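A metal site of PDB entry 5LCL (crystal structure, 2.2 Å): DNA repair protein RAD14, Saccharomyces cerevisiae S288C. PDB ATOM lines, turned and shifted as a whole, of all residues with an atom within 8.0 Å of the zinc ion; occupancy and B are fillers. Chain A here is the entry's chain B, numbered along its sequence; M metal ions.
ND2 of Asn 197 lies close to SG of Cys 213, at 3.3 Å. The side-chain sulfur (SG) of Cys 191 lies close to the backbone NH (N) of Glu 193 (3.3 Å). The backbone NH of Cys 191 sits at hydrogen-bond distance from the backbone carbonyl oxygen of Asn 197 (2.9 Å). A ring nitrogen (ND1) of His 195 sits close to the backbone carbonyl oxygen (O) of Cys 191. The side-chain sulfur (SG) of Cys 194 sits close to the backbone NH (N) of Asn 197, at 3.4 Å. SG of Cys 194 sits close to N of Ile 196.
The side-chain sulfur (SG) of Cys 216 is bound to the zinc ion, 2.3 Å away. The side-chain sulfur (SG) of Cys 213 is bound to the zinc ion. SG of Cys 191 is bound to the zinc ion. SG of Cys 194 binds the zinc ion, 2.4 Å away.
Within 4 Å of the zinc ion: Cys 191, Cys 194, Cys 213 and Cys 216. The nearest printed residue that does not touch the zinc ion is Glu 193 (4.5 Å).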
ATOM      1  N   LYS A 190      14.308   1.676 -16.847  1.00  0.00           N
ATOM      2  CA  LYS A 190      13.436   2.415 -17.751  1.00  0.00           C
ATOM      3  C   LYS A 190      11.996   2.467 -17.268  1.00  0.00           C
ATOM      4  O   LYS A 190      11.492   1.551 -16.640  1.00  0.00           O
ATOM      5  CB  LYS A 190      13.523   1.781 -19.158  1.00  0.00           C
ATOM      6  CG  LYS A 190      14.891   2.008 -19.815  1.00  0.00           C
ATOM      7  CD  LYS A 190      15.024   1.248 -21.102  1.00  0.00           C
ATOM      8  CE  LYS A 190      16.496   1.101 -21.488  1.00  0.00           C
ATOM      9  NZ  LYS A 190      17.190   2.437 -21.635  1.00  0.00           N
ATOM     10  N   CYS A 191      11.338   3.576 -17.550  1.00  0.00           N
ATOM     11  CA  CYS A 191       9.916   3.716 -17.297  1.00  0.00           C
ATOM     12  C   CYS A 191       9.147   2.543 -17.883  1.00  0.00           C
ATOM     13  O   CYS A 191       9.380   2.069 -18.974  1.00  0.00           O
ATOM     14  CB  CYS A 191       9.401   5.039 -17.865  1.00  0.00           C
ATOM     15  SG  CYS A 191       7.616   5.264 -17.935  1.00  0.00           S
ATOM     16  N   ILE A 192       8.242   2.033 -17.071  1.00  0.00           N
ATOM     17  CA  ILE A 192       7.467   0.868 -17.437  1.00  0.00           C
ATOM     18  C   ILE A 192       6.367   1.182 -18.476  1.00  0.00           C
ATOM     19  O   ILE A 192       5.782   0.234 -18.969  1.00  0.00           O
ATOM     20  CB  ILE A 192       6.793   0.266 -16.193  1.00  0.00           C
ATOM     21  CG1 ILE A 192       5.742   1.253 -15.641  1.00  0.00           C
ATOM     22  CG2 ILE A 192       7.816  -0.158 -15.148  1.00  0.00           C
ATOM     23  CD1 ILE A 192       5.133   0.846 -14.309  1.00  0.00           C
ATOM     24  N   GLU A 193       6.053   2.454 -18.775  1.00  0.00           N
ATOM     25  CA  GLU A 193       5.021   2.736 -19.773  1.00  0.00           C
ATOM     26  C   GLU A 193       5.676   2.947 -21.068  1.00  0.00           C
ATOM     27  O   GLU A 193       5.298   2.312 -22.017  1.00  0.00           O
ATOM     28  CB  GLU A 193       4.212   3.963 -19.447  1.00  0.00           C
ATOM     29  CG  GLU A 193       3.209   3.797 -18.353  1.00  0.00           C
ATOM     30  CD  GLU A 193       2.070   2.857 -18.675  1.00  0.00           C
ATOM     31  OE1 GLU A 193       1.480   2.384 -17.718  1.00  0.00           O
ATOM     32  OE2 GLU A 193       1.740   2.557 -19.854  1.00  0.00           O
ATOM     33  N   CYS A 194       6.657   3.877 -21.132  1.00  0.00           N
ATOM     34  CA  CYS A 194       7.353   4.168 -22.394  1.00  0.00           C
ATOM     35  C   CYS A 194       8.568   3.287 -22.656  1.00  0.00           C
ATOM     36  O   CYS A 194       8.979   3.141 -23.842  1.00  0.00           O
ATOM     37  CB  CYS A 194       7.753   5.624 -22.524  1.00  0.00           C
ATOM     38  SG  CYS A 194       8.930   6.268 -21.329  1.00  0.00           S
ATOM     39  N   HIS A 195       9.166   2.701 -21.624  1.00  0.00           N
ATOM     40  CA  HIS A 195      10.486   1.998 -21.785  1.00  0.00           C
ATOM     41  C   HIS A 195      11.592   2.863 -22.388  1.00  0.00           C
ATOM     42  O   HIS A 195      12.568   2.328 -22.980  1.00  0.00           O
ATOM     43  CB  HIS A 195      10.341   0.712 -22.626  1.00  0.00           C
ATOM     44  CG  HIS A 195       9.203  -0.126 -22.181  1.00  0.00           C
ATOM     45  ND1 HIS A 195       9.129  -0.635 -20.905  1.00  0.00           N
ATOM     46  CD2 HIS A 195       8.058  -0.483 -22.812  1.00  0.00           C
ATOM     47  CE1 HIS A 195       7.994  -1.309 -20.771  1.00  0.00           C
ATOM     48  NE2 HIS A 195       7.335  -1.240 -21.922  1.00  0.00           N
ATOM     49  N   ILE A 196      11.482   4.173 -22.238  1.00  0.00           N
ATOM     50  CA  ILE A 196      12.498   5.039 -22.803  1.00  0.00           C
ATOM     51  C   ILE A 196      13.102   5.897 -21.732  1.00  0.00           C
ATOM     52  O   ILE A 196      14.323   5.906 -21.568  1.00  0.00           O
ATOM     53  CB  ILE A 196      11.910   5.856 -23.964  1.00  0.00           C
ATOM     54  CG1 ILE A 196      11.603   4.914 -25.142  1.00  0.00           C
ATOM     55  CG2 ILE A 196      12.886   6.937 -24.420  1.00  0.00           C
ATOM     56  CD1 ILE A 196      10.638   5.507 -26.159  1.00  0.00           C
ATOM     57  N   ASN A 197      12.259   6.628 -20.992  1.00  0.00           N
ATOM     58  CA  ASN A 197      12.769   7.520 -19.950  1.00  0.00           C
ATOM     59  C   ASN A 197      13.399   6.760 -18.803  1.00  0.00           C
ATOM     60  O   ASN A 197      13.082   5.624 -18.514  1.00  0.00           O
ATOM     61  CB  ASN A 197      11.760   8.562 -19.435  1.00  0.00           C
ATOM     62  CG  ASN A 197      11.646   9.766 -20.349  1.00  0.00           C
ATOM     63  OD1 ASN A 197      12.667  10.283 -20.884  1.00  0.00           O
ATOM     64  ND2 ASN A 197      10.412  10.260 -20.522  1.00  0.00           N
ATOM     65  N   ILE A 198      14.322   7.448 -18.203  1.00  0.00           N
ATOM     66  CA  ILE A 198      15.187   6.943 -17.221  1.00  0.00           C
ATOM     67  C   ILE A 198      15.016   7.812 -15.934  1.00  0.00           C
ATOM     68  O   ILE A 198      15.501   7.377 -14.905  1.00  0.00           O
ATOM     69  CB  ILE A 198      16.601   6.956 -17.879  1.00  0.00           C
ATOM     70  CG1 ILE A 198      17.205   5.575 -17.915  1.00  0.00           C
ATOM     71  CG2 ILE A 198      17.543   8.025 -17.353  1.00  0.00           C
ATOM     72  CD1 ILE A 198      17.497   5.100 -19.329  1.00  0.00           C
ATOM     73  N   GLU A 199      14.347   8.983 -15.967  1.00  0.00           N
ATOM     74  CA  GLU A 199      14.142   9.779 -14.749  1.00  0.00           C
ATOM     75  C   GLU A 199      12.685   9.681 -14.443  1.00  0.00           C
ATOM     76  O   GLU A 199      11.822  10.055 -15.247  1.00  0.00           O
ATOM     77  CB  GLU A 199      14.501  11.243 -14.827  1.00  0.00           C
ATOM     78  CG  GLU A 199      15.272  11.731 -16.010  1.00  0.00           C
ATOM     79  CD  GLU A 199      16.725  11.890 -15.778  1.00  0.00           C
ATOM     80  OE1 GLU A 199      17.379  10.947 -15.240  1.00  0.00           O
ATOM     81  OE2 GLU A 199      17.222  12.954 -16.224  1.00  0.00           O
ATOM     82  N   MET A 200      12.404   9.148 -13.279  1.00  0.00           N
ATOM     83  CA  MET A 200      11.083   8.779 -12.911  1.00  0.00           C
ATOM     84  C   MET A 200      10.437  10.005 -12.274  1.00  0.00           C
ATOM     85  O   MET A 200      11.091  10.969 -11.907  1.00  0.00           O
ATOM     86  CB  MET A 200      11.113   7.549 -12.014  1.00  0.00           C
ATOM     87  CG  MET A 200      11.851   6.417 -12.655  1.00  0.00           C
ATOM     88  SD  MET A 200      11.207   5.822 -14.247  1.00  0.00           S
ATOM     89  CE  MET A 200      12.744   5.285 -15.010  1.00  0.00           C
ATOM     90  N   GLN A 211       7.924   3.099 -11.051  1.00  0.00           N
ATOM     91  CA  GLN A 211       8.947   3.534 -12.017  1.00  0.00           C
ATOM     92  C   GLN A 211       8.234   4.073 -13.245  1.00  0.00           C
ATOM     93  O   GLN A 211       8.212   3.377 -14.279  1.00  0.00           O
ATOM     94  CB  GLN A 211       9.791   2.358 -12.559  1.00  0.00           C
ATOM     95  CG  GLN A 211      10.630   1.616 -11.605  1.00  0.00           C
ATOM     96  CD  GLN A 211      11.975   1.338 -12.219  1.00  0.00           C
ATOM     97  OE1 GLN A 211      12.087   0.925 -13.411  1.00  0.00           O
ATOM     98  NE2 GLN A 211      13.015   1.645 -11.445  1.00  0.00           N
ATOM     99  N   VAL A 212       7.674   5.281 -13.125  1.00  0.00           N
ATOM    100  CA  VAL A 212       6.901   5.921 -14.191  1.00  0.00           C
ATOM    101  C   VAL A 212       7.444   7.327 -14.360  1.00  0.00           C
ATOM    102  O   VAL A 212       7.636   8.019 -13.356  1.00  0.00           O
ATOM    103  CB  VAL A 212       5.399   6.004 -13.867  1.00  0.00           C
ATOM    104  CG1 VAL A 212       4.647   6.596 -15.030  1.00  0.00           C
ATOM    105  CG2 VAL A 212       4.827   4.606 -13.641  1.00  0.00           C
ATOM    106  N   CYS A 213       7.743   7.722 -15.611  1.00  0.00           N
ATOM    107  CA  CYS A 213       8.237   9.056 -15.868  1.00  0.00           C
ATOM    108  C   CYS A 213       7.045  10.003 -15.811  1.00  0.00           C
ATOM    109  O   CYS A 213       5.913   9.571 -15.970  1.00  0.00           O
ATOM    110  CB  CYS A 213       8.971   9.168 -17.212  1.00  0.00           C
ATOM    111  SG  CYS A 213       7.943   9.048 -18.686  1.00  0.00           S
ATOM    112  N   LYS A 214       7.314  11.286 -15.565  1.00  0.00           N
ATOM    113  CA  LYS A 214       6.258  12.276 -15.468  1.00  0.00           C
ATOM    114  C   LYS A 214       5.392  12.367 -16.732  1.00  0.00           C
ATOM    115  O   LYS A 214       4.162  12.513 -16.649  1.00  0.00           O
ATOM    116  CB  LYS A 214       6.833  13.662 -15.174  1.00  0.00           C
ATOM    117  CG  LYS A 214       5.770  14.682 -14.775  1.00  0.00           C
ATOM    118  CD  LYS A 214       6.353  16.075 -14.482  1.00  0.00           C
ATOM    119  CE  LYS A 214       6.248  17.010 -15.704  1.00  0.00           C
ATOM    120  NZ  LYS A 214       6.615  18.485 -15.499  1.00  0.00           N
ATOM    121  N   GLN A 215       6.016  12.295 -17.901  1.00  0.00           N
ATOM    122  CA  GLN A 215       5.253  12.422 -19.134  1.00  0.00           C
ATOM    123  C   GLN A 215       4.246  11.271 -19.284  1.00  0.00           C
ATOM    124  O   GLN A 215       3.110  11.508 -19.618  1.00  0.00           O
ATOM    125  CB  GLN A 215       6.196  12.557 -20.352  1.00  0.00           C
ATOM    126  CG  GLN A 215       5.491  12.448 -21.700  1.00  0.00           C
ATOM    127  CD  GLN A 215       6.423  12.711 -22.848  1.00  0.00           C
ATOM    128  OE1 GLN A 215       7.627  12.900 -22.677  1.00  0.00           O
ATOM    129  NE2 GLN A 215       5.872  12.740 -24.044  1.00  0.00           N
ATOM    130  N   CYS A 216       4.658  10.035 -19.027  1.00  0.00           N
ATOM    131  CA  CYS A 216       3.741   8.894 -19.053  1.00  0.00           C
ATOM    132  C   CYS A 216       2.615   9.062 -18.015  1.00  0.00           C
ATOM    133  O   CYS A 216       1.472   8.623 -18.245  1.00  0.00           O
ATOM    134  CB  CYS A 216       4.500   7.575 -18.897  1.00  0.00           C
ATOM    135  SG  CYS A 216       5.461   7.212 -20.383  1.00  0.00           S
ATOM    136  N   SER A 217       2.904   9.739 -16.907  1.00  0.00           N
ATOM    137  CA  SER A 217       1.879   9.909 -15.878  1.00  0.00           C
ATOM    138  C   SER A 217       0.770  10.827 -16.347  1.00  0.00           C
ATOM    139  O   SER A 217      -0.381  10.528 -16.072  1.00  0.00           O
ATOM    140  CB  SER A 217       2.462  10.370 -14.547  1.00  0.00           C
ATOM    141  OG  SER A 217       2.637  11.752 -14.496  1.00  0.00           O
ATOM    142  N   GLU A 219       0.137  11.220 -19.515  1.00  0.00           N
ATOM    143  CA  GLU A 219      -0.476  10.513 -20.621  1.00  0.00           C
ATOM    144  C   GLU A 219      -1.405   9.373 -20.189  1.00  0.00           C
ATOM    145  O   GLU A 219      -2.113   8.834 -21.002  1.00  0.00           O
ATOM    146  CB  GLU A 219       0.610   9.990 -21.571  1.00  0.00           C
ATOM    147  CG  GLU A 219       1.372  11.124 -22.265  1.00  0.00           C
ATOM    148  CD  GLU A 219       2.627  10.707 -23.041  1.00  0.00           C
ATOM    149  OE1 GLU A 219       3.202   9.634 -22.798  1.00  0.00           O
ATOM    150  OE2 GLU A 219       3.067  11.529 -23.881  1.00  0.00           O
ATOM    151  N   HIS A 220      -1.390   8.962 -18.908  1.00  0.00           N
ATOM    152  CA  HIS A 220      -2.246   7.873 -18.511  1.00  0.00           C
ATOM    153  C   HIS A 220      -2.836   8.138 -17.168  1.00  0.00           C
ATOM    154  O   HIS A 220      -2.584   7.383 -16.201  1.00  0.00           O
ATOM    155  CB  HIS A 220      -1.431   6.618 -18.486  1.00  0.00           C
ATOM    156  CG  HIS A 220      -0.926   6.189 -19.822  1.00  0.00           C
ATOM    157  ND1 HIS A 220      -1.732   5.604 -20.754  1.00  0.00           N
ATOM    158  CD2 HIS A 220       0.306   6.259 -20.375  1.00  0.00           C
ATOM    159  CE1 HIS A 220      -1.030   5.317 -21.829  1.00  0.00           C
ATOM    160  NE2 HIS A 220       0.210   5.701 -21.616  1.00  0.00           N
ATOM    161  N   TYR A 224      -2.415   6.874 -13.287  1.00  0.00           N
ATOM    162  CA  TYR A 224      -1.466   7.623 -12.495  1.00  0.00           C
ATOM    163  C   TYR A 224      -1.975   8.900 -11.882  1.00  0.00           C
ATOM    164  O   TYR A 224      -1.230   9.530 -11.150  1.00  0.00           O
ATOM    165  CB  TYR A 224      -0.204   7.906 -13.292  1.00  0.00           C
ATOM    166  CG  TYR A 224       0.346   6.629 -13.854  1.00  0.00           C
ATOM    167  CD1 TYR A 224       0.739   5.615 -13.020  1.00  0.00           C
ATOM    168  CD2 TYR A 224       0.433   6.409 -15.182  1.00  0.00           C
ATOM    169  CE1 TYR A 224       1.233   4.413 -13.511  1.00  0.00           C
ATOM    170  CE2 TYR A 224       0.912   5.194 -15.673  1.00  0.00           C
ATOM    171  CZ  TYR A 224       1.287   4.187 -14.812  1.00  0.00           C
ATOM    172  OH  TYR A 224       1.787   2.964 -15.279  1.00  0.00           O
HETATM  173 ZN    ZN M   1       7.530   6.935 -19.536  1.00  0.00          ZN
